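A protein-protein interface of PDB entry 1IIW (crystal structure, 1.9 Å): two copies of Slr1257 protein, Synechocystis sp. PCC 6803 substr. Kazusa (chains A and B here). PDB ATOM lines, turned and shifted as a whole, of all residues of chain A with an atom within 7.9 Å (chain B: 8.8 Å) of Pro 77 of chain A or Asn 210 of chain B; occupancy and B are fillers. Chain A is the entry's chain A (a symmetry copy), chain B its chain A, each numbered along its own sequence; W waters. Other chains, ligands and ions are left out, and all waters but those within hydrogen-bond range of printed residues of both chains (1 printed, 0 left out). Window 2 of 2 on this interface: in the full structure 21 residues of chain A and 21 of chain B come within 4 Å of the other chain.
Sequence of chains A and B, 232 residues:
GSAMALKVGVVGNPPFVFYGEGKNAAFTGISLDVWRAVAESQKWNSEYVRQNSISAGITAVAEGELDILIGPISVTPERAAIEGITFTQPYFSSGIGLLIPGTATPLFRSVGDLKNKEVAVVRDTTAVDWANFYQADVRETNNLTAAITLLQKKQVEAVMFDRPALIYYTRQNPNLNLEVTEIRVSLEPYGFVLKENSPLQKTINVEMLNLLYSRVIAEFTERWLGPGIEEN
Water W1 lies within hydrogen-bond range of the backbone carbonyl oxygen (O) of Phe 87 of chain A (2.8 Å), the side-chain amide nitrogen (NE2) of Gln 89 of chain B (3.1 Å) and the side-chain amide nitrogen (ND2) of Asn 205 of chain B (3.3 Å).
The backbone carbonyl oxygen (O) of Val 206 of chain B is in hydrogen-bond range of the side-chain amide nitrogen (ND2) of Asn 210 of chain B (3.1 Å).
OD1 of Asn 205 of chain B is in hydrogen-bond range of N of Gln 89 of chain B (2.9 Å).
OE1 of Glu 207 of chain B lies within hydrogen-bond range of ND2 of Asn 210 of chain B.
The side-chain hydroxyl of Thr 76 of chain A sits at hydrogen-bond distance from the backbone NH of Arg 79 of chain A, at 3.2 Å.
The backbone carbonyl oxygen (O) of Asn 210 of chain B is in hydrogen-bond range of the side-chain hydroxyl (OG) of Ser 214 of chain B (2.7 Å).
CG1 of Val 75 of chain A touches OE1 of Gln 89 of chain B (3.7 Å).
CG1 of Val 75 of chain A touches CD1 of Leu 209 of chain B, at 3.7 Å.
Leu 209 of chain B touches Thr 76 of chain A.
OH of Tyr 213 of chain B touches CG2 of Thr 76 of chain A (3.96 Å).
Pro 77 of chain A touches Leu 209 of chain B.
Asn 210 of chain B touches Pro 77 of chain A.
Ala 80 of chain A touches Val 206 of chain B (C to CG2, 3.7 Å).
Leu 209 of chain B touches Ala 80 of chain A.
CG2 of Val 206 of chain B touches CA of Ala 81 of chain A (3.6 Å).
NE2 of Gln 89 of chain B touches CB of Phe 87 of chain A (3.8 Å).
No position is printed for both chains.
Of the printed residues of chain B, Val 75 of chain A touches Gln 89, Leu 209 and Tyr 213.
Thr 76 of chain A touches two residues of chain B.
Printed residues of chain B within 4 Å of Pro 77 of chain A: Val 206 (3.8 Å), Leu 209 (3.7 Å), Asn 210 (3.0 Å) and Tyr 213 (3.8 Å).
Printed residues of chain B within 4 Å of Ala 80 of chain A: Lys 202 (2.7 Å), Val 206 (3.7 Å) and Leu 209 (3.7 Å).
Printed residues of chain B within 4 Å of Ile 82 of chain A: Lys 202 (2.9 Å).
Of the printed residues of chain B, Phe 87 of chain A touches Gln 89.
Val 38 of chain B touches none of the printed residues of chain A.
Printed residues of chain A within 4 Å of Val 206 of chain B: Pro 77 (3.8 Å), Ala 80 (3.7 Å) and Ala 81 (3.6 Å).
Of chain A, only Pro 77 comes within 4 Å of Asn 210 of chain B.
Hydrophobic or aromatic side chains of chain B within 4 Å of the printed part of chain A: Val 206, Leu 209 and Tyr 213.
Among the printed residues, 16 pairs touch across the chains.
Among the printed residues, no Asp or Glu carboxylate lies within 4 Å of a Lys or Arg side-chain nitrogen of the other chain.
The side-chain amino group (NZ) of Lys 202 of chain B sits at hydrogen-bond distance from the backbone carbonyl oxygen (O) of Ile 85 of chain A, at 2.6 Å.
The side-chain hydroxyl (OH) of Tyr 213 of chain B lies within hydrogen-bond range of the backbone carbonyl oxygen (O) of Val 75 of chain A (2.6 Å).
The backbone carbonyl oxygen of Ile 82 of chain A lies within hydrogen-bond range of the side-chain amino group of Lys 202 of chain B (2.9 Å).
NZ of Lys 202 of chain B is in hydrogen-bond range of O of Ala 80 of chain A (2.7 Å).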
ATOM      1  N   SER A  74      11.250 -26.604  -9.446  1.00  0.00           N
ATOM      2  CA  SER A  74      10.816 -25.502  -8.592  1.00  0.00           C
ATOM      3  C   SER A  74      10.138 -25.995  -7.325  1.00  0.00           C
ATOM      4  O   SER A  74       9.288 -26.891  -7.366  1.00  0.00           O
ATOM      5  CB  SER A  74       9.835 -24.602  -9.337  1.00  0.00           C
ATOM      6  OG  SER A  74      10.458 -23.998 -10.445  1.00  0.00           O
ATOM      7  N   VAL A  75      10.540 -25.415  -6.202  1.00  0.00           N
ATOM      8  CA  VAL A  75       9.956 -25.748  -4.905  1.00  0.00           C
ATOM      9  C   VAL A  75       8.686 -24.919  -4.757  1.00  0.00           C
ATOM     10  O   VAL A  75       8.756 -23.703  -4.567  1.00  0.00           O
ATOM     11  CB  VAL A  75      10.893 -25.384  -3.741  1.00  0.00           C
ATOM     12  CG1 VAL A  75      10.340 -25.957  -2.445  1.00  0.00           C
ATOM     13  CG2 VAL A  75      12.298 -25.892  -4.003  1.00  0.00           C
ATOM     14  N   THR A  76       7.538 -25.575  -4.906  1.00  0.00           N
ATOM     15  CA  THR A  76       6.229 -24.918  -4.794  1.00  0.00           C
ATOM     16  C   THR A  76       5.422 -25.552  -3.661  1.00  0.00           C
ATOM     17  O   THR A  76       5.707 -26.673  -3.240  1.00  0.00           O
ATOM     18  CB  THR A  76       5.395 -25.058  -6.101  1.00  0.00           C
ATOM     19  OG1 THR A  76       5.016 -26.428  -6.282  1.00  0.00           O
ATOM     20  CG2 THR A  76       6.195 -24.588  -7.320  1.00  0.00           C
ATOM     21  N   PRO A  77       4.390 -24.845  -3.163  1.00  0.00           N
ATOM     22  CA  PRO A  77       3.548 -25.364  -2.077  1.00  0.00           C
ATOM     23  C   PRO A  77       2.885 -26.691  -2.469  1.00  0.00           C
ATOM     24  O   PRO A  77       2.852 -27.643  -1.688  1.00  0.00           O
ATOM     25  CB  PRO A  77       2.498 -24.269  -1.914  1.00  0.00           C
ATOM     26  CG  PRO A  77       3.204 -23.032  -2.356  1.00  0.00           C
ATOM     27  CD  PRO A  77       3.978 -23.486  -3.553  1.00  0.00           C
ATOM     28  N   GLU A  78       2.389 -26.754  -3.699  1.00  0.00           N
ATOM     29  CA  GLU A  78       1.719 -27.946  -4.200  1.00  0.00           C
ATOM     30  C   GLU A  78       2.642 -29.163  -4.265  1.00  0.00           C
ATOM     31  O   GLU A  78       2.252 -30.266  -3.881  1.00  0.00           O
ATOM     32  CB  GLU A  78       1.086 -27.660  -5.575  1.00  0.00           C
ATOM     33  N   ARG A  79       3.873 -28.964  -4.723  1.00  0.00           N
ATOM     34  CA  ARG A  79       4.811 -30.070  -4.822  1.00  0.00           C
ATOM     35  C   ARG A  79       5.318 -30.521  -3.457  1.00  0.00           C
ATOM     36  O   ARG A  79       5.482 -31.717  -3.211  1.00  0.00           O
ATOM     37  CB  ARG A  79       5.973 -29.708  -5.747  1.00  0.00           C
ATOM     38  CG  ARG A  79       5.554 -29.620  -7.199  1.00  0.00           C
ATOM     39  CD  ARG A  79       6.697 -29.232  -8.108  1.00  0.00           C
ATOM     40  NE  ARG A  79       6.223 -29.011  -9.473  1.00  0.00           N
ATOM     41  CZ  ARG A  79       6.889 -28.318 -10.388  1.00  0.00           C
ATOM     42  NH1 ARG A  79       8.060 -27.769 -10.093  1.00  0.00           N
ATOM     43  NH2 ARG A  79       6.396 -28.195 -11.612  1.00  0.00           N
ATOM     44  N   ALA A  80       5.545 -29.563  -2.563  1.00  0.00           N
ATOM     45  CA  ALA A  80       6.033 -29.872  -1.224  1.00  0.00           C
ATOM     46  C   ALA A  80       4.942 -30.573  -0.418  1.00  0.00           C
ATOM     47  O   ALA A  80       5.237 -31.278   0.543  1.00  0.00           O
ATOM     48  CB  ALA A  80       6.482 -28.595  -0.512  1.00  0.00           C
ATOM     49  N   ALA A  81       3.692 -30.393  -0.832  1.00  0.00           N
ATOM     50  CA  ALA A  81       2.552 -31.007  -0.153  1.00  0.00           C
ATOM     51  C   ALA A  81       2.350 -32.478  -0.516  1.00  0.00           C
ATOM     52  O   ALA A  81       1.586 -33.180   0.146  1.00  0.00           O
ATOM     53  CB  ALA A  81       1.276 -30.219  -0.437  1.00  0.00           C
ATOM     54  N   ILE A  82       3.025 -32.943  -1.563  1.00  0.00           N
ATOM     55  CA  ILE A  82       2.893 -34.330  -1.989  1.00  0.00           C
ATOM     56  C   ILE A  82       3.428 -35.242  -0.886  1.00  0.00           C
ATOM     57  O   ILE A  82       4.505 -35.005  -0.342  1.00  0.00           O
ATOM     58  CB  ILE A  82       3.635 -34.579  -3.334  1.00  0.00           C
ATOM     59  CG1 ILE A  82       2.920 -33.828  -4.458  1.00  0.00           C
ATOM     60  CG2 ILE A  82       3.694 -36.074  -3.663  1.00  0.00           C
ATOM     61  CD1 ILE A  82       3.705 -33.755  -5.760  1.00  0.00           C
ATOM     62  N   ILE A  85       7.499 -37.265  -0.001  1.00  0.00           N
ATOM     63  CA  ILE A  85       8.692 -36.608  -0.504  1.00  0.00           C
ATOM     64  C   ILE A  85       9.088 -35.387   0.320  1.00  0.00           C
ATOM     65  O   ILE A  85       8.326 -34.900   1.151  1.00  0.00           O
ATOM     66  CB  ILE A  85       8.553 -36.194  -2.004  1.00  0.00           C
ATOM     67  CG1 ILE A  85       7.388 -35.222  -2.204  1.00  0.00           C
ATOM     68  CG2 ILE A  85       8.402 -37.423  -2.892  1.00  0.00           C
ATOM     69  CD1 ILE A  85       7.764 -33.761  -2.081  1.00  0.00           C
ATOM     70  N   PHE A  87      11.803 -31.801  -0.372  1.00  0.00           N
ATOM     71  CA  PHE A  87      12.775 -31.090  -1.202  1.00  0.00           C
ATOM     72  C   PHE A  87      14.086 -30.838  -0.471  1.00  0.00           C
ATOM     73  O   PHE A  87      14.100 -30.681   0.751  1.00  0.00           O
ATOM     74  CB  PHE A  87      12.217 -29.734  -1.611  1.00  0.00           C
ATOM     75  CG  PHE A  87      11.316 -29.783  -2.794  1.00  0.00           C
ATOM     76  CD1 PHE A  87       9.958 -30.019  -2.636  1.00  0.00           C
ATOM     77  CD2 PHE A  87      11.818 -29.553  -4.070  1.00  0.00           C
ATOM     78  CE1 PHE A  87       9.107 -30.026  -3.732  1.00  0.00           C
ATOM     79  CE2 PHE A  87      10.980 -29.557  -5.176  1.00  0.00           C
ATOM     80  CZ  PHE A  87       9.619 -29.790  -5.011  1.00  0.00           C
ATOM     81  N   THR A 126       5.012 -25.021 -13.808  1.00  0.00           N
ATOM     82  CA  THR A 126       4.389 -23.984 -12.997  1.00  0.00           C
ATOM     83  C   THR A 126       3.751 -22.889 -13.853  1.00  0.00           C
ATOM     84  O   THR A 126       2.823 -22.212 -13.418  1.00  0.00           O
ATOM     85  CB  THR A 126       5.412 -23.353 -12.036  1.00  0.00           C
ATOM     86  OG1 THR A 126       6.493 -22.793 -12.790  1.00  0.00           O
ATOM     87  CG2 THR A 126       5.967 -24.406 -11.065  1.00  0.00           C
ATOM     88  N   ALA B  37       1.838 -16.658  11.354  1.00  0.00           N
ATOM     89  CA  ALA B  37       0.942 -16.940  10.233  1.00  0.00           C
ATOM     90  C   ALA B  37       0.862 -18.464  10.046  1.00  0.00           C
ATOM     91  O   ALA B  37      -0.211 -19.020   9.810  1.00  0.00           O
ATOM     92  CB  ALA B  37       1.450 -16.267   8.965  1.00  0.00           C
ATOM     93  N   VAL B  38       2.007 -19.130  10.176  1.00  0.00           N
ATOM     94  CA  VAL B  38       2.086 -20.581  10.047  1.00  0.00           C
ATOM     95  C   VAL B  38       1.284 -21.263  11.162  1.00  0.00           C
ATOM     96  O   VAL B  38       0.497 -22.170  10.896  1.00  0.00           O
ATOM     97  CB  VAL B  38       3.552 -21.064  10.115  1.00  0.00           C
ATOM     98  CG1 VAL B  38       3.621 -22.592  10.245  1.00  0.00           C
ATOM     99  CG2 VAL B  38       4.308 -20.599   8.876  1.00  0.00           C
ATOM    100  N   SER B  41      -2.581 -20.728  10.803  1.00  0.00           N
ATOM    101  CA  SER B  41      -3.181 -21.516   9.726  1.00  0.00           C
ATOM    102  C   SER B  41      -3.482 -22.952  10.161  1.00  0.00           C
ATOM    103  O   SER B  41      -4.364 -23.605   9.600  1.00  0.00           O
ATOM    104  CB  SER B  41      -2.290 -21.522   8.476  1.00  0.00           C
ATOM    105  OG  SER B  41      -1.153 -22.352   8.650  1.00  0.00           O
ATOM    106  N   GLN B  42      -2.774 -23.421  11.184  1.00  0.00           N
ATOM    107  CA  GLN B  42      -2.954 -24.773  11.696  1.00  0.00           C
ATOM    108  C   GLN B  42      -3.626 -24.788  13.063  1.00  0.00           C
ATOM    109  O   GLN B  42      -3.864 -25.855  13.626  1.00  0.00           O
ATOM    110  CB  GLN B  42      -1.597 -25.483  11.796  1.00  0.00           C
ATOM    111  CG  GLN B  42      -0.802 -25.512  10.496  1.00  0.00           C
ATOM    112  CD  GLN B  42      -1.582 -26.139   9.366  1.00  0.00           C
ATOM    113  OE1 GLN B  42      -2.065 -27.263   9.483  1.00  0.00           O
ATOM    114  NE2 GLN B  42      -1.716 -25.415   8.263  1.00  0.00           N
ATOM    115  N   GLN B  89      12.464 -24.871   4.391  1.00  0.00           N
ATOM    116  CA  GLN B  89      12.808 -24.204   3.141  1.00  0.00           C
ATOM    117  C   GLN B  89      13.055 -22.735   3.544  1.00  0.00           C
ATOM    118  O   GLN B  89      12.452 -22.252   4.498  1.00  0.00           O
ATOM    119  CB  GLN B  89      11.629 -24.275   2.174  1.00  0.00           C
ATOM    120  CG  GLN B  89      11.562 -25.561   1.385  1.00  0.00           C
ATOM    121  CD  GLN B  89      12.739 -25.694   0.456  1.00  0.00           C
ATOM    122  OE1 GLN B  89      13.051 -24.769  -0.282  1.00  0.00           O
ATOM    123  NE2 GLN B  89      13.427 -26.832   0.511  1.00  0.00           N
ATOM    124  N   LYS B 202       6.638 -31.100   6.857  1.00  0.00           N
ATOM    125  CA  LYS B 202       5.887 -30.902   5.626  1.00  0.00           C
ATOM    126  C   LYS B 202       4.842 -29.813   5.771  1.00  0.00           C
ATOM    127  O   LYS B 202       4.702 -28.972   4.889  1.00  0.00           O
ATOM    128  CB  LYS B 202       5.246 -32.214   5.149  1.00  0.00           C
ATOM    129  CG  LYS B 202       4.519 -32.095   3.807  1.00  0.00           C
ATOM    130  CD  LYS B 202       4.146 -33.454   3.216  1.00  0.00           C
ATOM    131  CE  LYS B 202       5.377 -34.233   2.748  1.00  0.00           C
ATOM    132  NZ  LYS B 202       6.132 -33.573   1.647  1.00  0.00           N
ATOM    133  N   THR B 203       4.136 -29.802   6.899  1.00  0.00           N
ATOM    134  CA  THR B 203       3.102 -28.797   7.135  1.00  0.00           C
ATOM    135  C   THR B 203       3.707 -27.405   7.171  1.00  0.00           C
ATOM    136  O   THR B 203       3.175 -26.469   6.563  1.00  0.00           O
ATOM    137  CB  THR B 203       2.357 -29.048   8.457  1.00  0.00           C
ATOM    138  OG1 THR B 203       1.652 -30.288   8.374  1.00  0.00           O
ATOM    139  CG2 THR B 203       1.363 -27.931   8.728  1.00  0.00           C
ATOM    140  N   ILE B 204       4.828 -27.282   7.878  1.00  0.00           N
ATOM    141  CA  ILE B 204       5.523 -26.003   8.003  1.00  0.00           C
ATOM    142  C   ILE B 204       6.079 -25.547   6.650  1.00  0.00           C
ATOM    143  O   ILE B 204       5.880 -24.400   6.252  1.00  0.00           O
ATOM    144  CB  ILE B 204       6.632 -26.076   9.085  1.00  0.00           C
ATOM    145  CG1 ILE B 204       5.976 -26.245  10.465  1.00  0.00           C
ATOM    146  CG2 ILE B 204       7.492 -24.818   9.056  1.00  0.00           C
ATOM    147  CD1 ILE B 204       6.952 -26.336  11.610  1.00  0.00           C
ATOM    148  N   ASN B 205       6.718 -26.461   5.923  1.00  0.00           N
ATOM    149  CA  ASN B 205       7.271 -26.128   4.607  1.00  0.00           C
ATOM    150  C   ASN B 205       6.208 -25.641   3.633  1.00  0.00           C
ATOM    151  O   ASN B 205       6.364 -24.587   3.026  1.00  0.00           O
ATOM    152  CB  ASN B 205       8.036 -27.314   4.012  1.00  0.00           C
ATOM    153  CG  ASN B 205       9.458 -27.405   4.535  1.00  0.00           C
ATOM    154  OD1 ASN B 205      10.060 -26.393   4.891  1.00  0.00           O
ATOM    155  ND2 ASN B 205      10.000 -28.616   4.586  1.00  0.00           N
ATOM    156  N   VAL B 206       5.105 -26.381   3.536  1.00  0.00           N
ATOM    157  CA  VAL B 206       4.009 -26.022   2.639  1.00  0.00           C
ATOM    158  C   VAL B 206       3.431 -24.643   2.977  1.00  0.00           C
ATOM    159  O   VAL B 206       3.166 -23.838   2.081  1.00  0.00           O
ATOM    160  CB  VAL B 206       2.888 -27.101   2.661  1.00  0.00           C
ATOM    161  CG1 VAL B 206       1.719 -26.685   1.795  1.00  0.00           C
ATOM    162  CG2 VAL B 206       3.445 -28.434   2.187  1.00  0.00           C
ATOM    163  N   GLU B 207       3.274 -24.362   4.268  1.00  0.00           N
ATOM    164  CA  GLU B 207       2.729 -23.087   4.713  1.00  0.00           C
ATOM    165  C   GLU B 207       3.659 -21.921   4.433  1.00  0.00           C
ATOM    166  O   GLU B 207       3.220 -20.857   3.994  1.00  0.00           O
ATOM    167  CB  GLU B 207       2.416 -23.126   6.213  1.00  0.00           C
ATOM    168  CG  GLU B 207       0.942 -23.159   6.519  1.00  0.00           C
ATOM    169  CD  GLU B 207       0.163 -22.123   5.726  1.00  0.00           C
ATOM    170  OE1 GLU B 207      -0.575 -22.544   4.816  1.00  0.00           O
ATOM    171  OE2 GLU B 207       0.300 -20.902   5.995  1.00  0.00           O
ATOM    172  N   MET B 208       4.938 -22.111   4.738  1.00  0.00           N
ATOM    173  CA  MET B 208       5.933 -21.076   4.512  1.00  0.00           C
ATOM    174  C   MET B 208       6.012 -20.758   3.023  1.00  0.00           C
ATOM    175  O   MET B 208       6.100 -19.595   2.635  1.00  0.00           O
ATOM    176  CB  MET B 208       7.290 -21.509   5.063  1.00  0.00           C
ATOM    177  CG  MET B 208       7.394 -21.359   6.579  1.00  0.00           C
ATOM    178  SD  MET B 208       8.917 -22.026   7.246  1.00  0.00           S
ATOM    179  CE  MET B 208      10.083 -20.780   6.769  1.00  0.00           C
ATOM    180  N   LEU B 209       5.919 -21.795   2.199  1.00  0.00           N
ATOM    181  CA  LEU B 209       5.949 -21.639   0.753  1.00  0.00           C
ATOM    182  C   LEU B 209       4.695 -20.898   0.273  1.00  0.00           C
ATOM    183  O   LEU B 209       4.781 -20.069  -0.634  1.00  0.00           O
ATOM    184  CB  LEU B 209       6.116 -23.001   0.066  1.00  0.00           C
ATOM    185  CG  LEU B 209       7.509 -23.634   0.226  1.00  0.00           C
ATOM    186  CD1 LEU B 209       7.488 -25.081  -0.216  1.00  0.00           C
ATOM    187  CD2 LEU B 209       8.549 -22.830  -0.552  1.00  0.00           C
ATOM    188  N   ASN B 210       3.545 -21.161   0.898  1.00  0.00           N
ATOM    189  CA  ASN B 210       2.306 -20.455   0.541  1.00  0.00           C
ATOM    190  C   ASN B 210       2.447 -18.962   0.828  1.00  0.00           C
ATOM    191  O   ASN B 210       2.053 -18.127   0.018  1.00  0.00           O
ATOM    192  CB  ASN B 210       1.101 -20.976   1.332  1.00  0.00           C
ATOM    193  CG  ASN B 210       0.568 -22.266   0.793  1.00  0.00           C
ATOM    194  OD1 ASN B 210       0.543 -22.478  -0.413  1.00  0.00           O
ATOM    195  ND2 ASN B 210       0.129 -23.144   1.689  1.00  0.00           N
ATOM    196  N   LEU B 211       2.989 -18.637   1.999  1.00  0.00           N
ATOM    197  CA  LEU B 211       3.189 -17.248   2.412  1.00  0.00           C
ATOM    198  C   LEU B 211       4.206 -16.560   1.511  1.00  0.00           C
ATOM    199  O   LEU B 211       4.097 -15.371   1.219  1.00  0.00           O
ATOM    200  CB  LEU B 211       3.671 -17.203   3.866  1.00  0.00           C
ATOM    201  CG  LEU B 211       2.711 -17.718   4.944  1.00  0.00           C
ATOM    202  CD1 LEU B 211       3.473 -17.977   6.235  1.00  0.00           C
ATOM    203  CD2 LEU B 211       1.596 -16.709   5.171  1.00  0.00           C
ATOM    204  N   LEU B 212       5.198 -17.327   1.081  1.00  0.00           N
ATOM    205  CA  LEU B 212       6.256 -16.837   0.212  1.00  0.00           C
ATOM    206  C   LEU B 212       5.708 -16.465  -1.161  1.00  0.00           C
ATOM    207  O   LEU B 212       5.877 -15.337  -1.618  1.00  0.00           O
ATOM    208  CB  LEU B 212       7.325 -17.915   0.056  1.00  0.00           C
ATOM    209  CG  LEU B 212       8.599 -17.564  -0.694  1.00  0.00           C
ATOM    210  CD1 LEU B 212       9.329 -16.442   0.049  1.00  0.00           C
ATOM    211  CD2 LEU B 212       9.470 -18.812  -0.802  1.00  0.00           C
ATOM    212  N   TYR B 213       5.044 -17.425  -1.803  1.00  0.00           N
ATOM    213  CA  TYR B 213       4.473 -17.227  -3.134  1.00  0.00           C
ATOM    214  C   TYR B 213       3.311 -16.233  -3.190  1.00  0.00           C
ATOM    215  O   TYR B 213       3.105 -15.572  -4.211  1.00  0.00           O
ATOM    216  CB  TYR B 213       4.052 -18.573  -3.725  1.00  0.00           C
ATOM    217  CG  TYR B 213       5.206 -19.369  -4.305  1.00  0.00           C
ATOM    218  CD1 TYR B 213       5.962 -20.226  -3.512  1.00  0.00           C
ATOM    219  CD2 TYR B 213       5.532 -19.268  -5.657  1.00  0.00           C
ATOM    220  CE1 TYR B 213       7.009 -20.966  -4.052  1.00  0.00           C
ATOM    221  CE2 TYR B 213       6.577 -20.000  -6.204  1.00  0.00           C
ATOM    222  CZ  TYR B 213       7.309 -20.847  -5.398  1.00  0.00           C
ATOM    223  OH  TYR B 213       8.348 -21.564  -5.941  1.00  0.00           O
ATOM    224  N   SER B 214       2.592 -16.089  -2.079  1.00  0.00           N
ATOM    225  CA  SER B 214       1.453 -15.180  -2.014  1.00  0.00           C
ATOM    226  C   SER B 214       1.851 -13.743  -1.722  1.00  0.00           C
ATOM    227  O   SER B 214       0.994 -12.876  -1.614  1.00  0.00           O
ATOM    228  CB  SER B 214       0.454 -15.651  -0.952  1.00  0.00           C
ATOM    229  OG  SER B 214       1.027 -15.662   0.341  1.00  0.00           O
ATOM    230  N   ARG B 215       3.153 -13.498  -1.604  1.00  0.00           N
ATOM    231  CA  ARG B 215       3.697 -12.167  -1.323  1.00  0.00           C
ATOM    232  C   ARG B 215       3.461 -11.725   0.120  1.00  0.00           C
ATOM    233  O   ARG B 215       3.741 -10.574   0.466  1.00  0.00           O
ATOM    234  CB  ARG B 215       3.097 -11.113  -2.266  1.00  0.00           C
ATOM    235  CG  ARG B 215       3.548 -11.193  -3.705  1.00  0.00           C
ATOM    236  CD  ARG B 215       5.040 -10.942  -3.801  1.00  0.00           C
ATOM    237  NE  ARG B 215       5.742 -12.176  -4.141  1.00  0.00           N
ATOM    238  CZ  ARG B 215       7.064 -12.341  -4.079  1.00  0.00           C
ATOM    239  NH1 ARG B 215       7.852 -11.340  -3.677  1.00  0.00           N
ATOM    240  NH2 ARG B 215       7.593 -13.515  -4.430  1.00  0.00           N
ATOM    241  N   VAL B 216       2.925 -12.621   0.950  1.00  0.00           N
ATOM    242  CA  VAL B 216       2.652 -12.294   2.351  1.00  0.00           C
ATOM    243  C   VAL B 216       3.931 -11.965   3.136  1.00  0.00           C
ATOM    244  O   VAL B 216       3.948 -11.026   3.947  1.00  0.00           O
ATOM    245  CB  VAL B 216       1.848 -13.418   3.038  1.00  0.00           C
ATOM    246  CG1 VAL B 216       1.874 -13.255   4.544  1.00  0.00           C
ATOM    247  CG2 VAL B 216       0.402 -13.388   2.551  1.00  0.00           C
ATOM    248  N   ILE B 217       5.001 -12.712   2.881  1.00  0.00           N
ATOM    249  CA  ILE B 217       6.264 -12.462   3.568  1.00  0.00           C
ATOM    250  C   ILE B 217       6.868 -11.143   3.092  1.00  0.00           C
ATOM    251  O   ILE B 217       7.495 -10.421   3.873  1.00  0.00           O
ATOM    252  CB  ILE B 217       7.273 -13.629   3.396  1.00  0.00           C
ATOM    253  CG1 ILE B 217       6.675 -14.931   3.942  1.00  0.00           C
ATOM    254  CG2 ILE B 217       8.566 -13.311   4.136  1.00  0.00           C
ATOM    255  CD1 ILE B 217       7.555 -16.137   3.783  1.00  0.00           C
HETATM  256  O   HOH W   1      12.350 -29.115   2.299  1.00  0.00           O
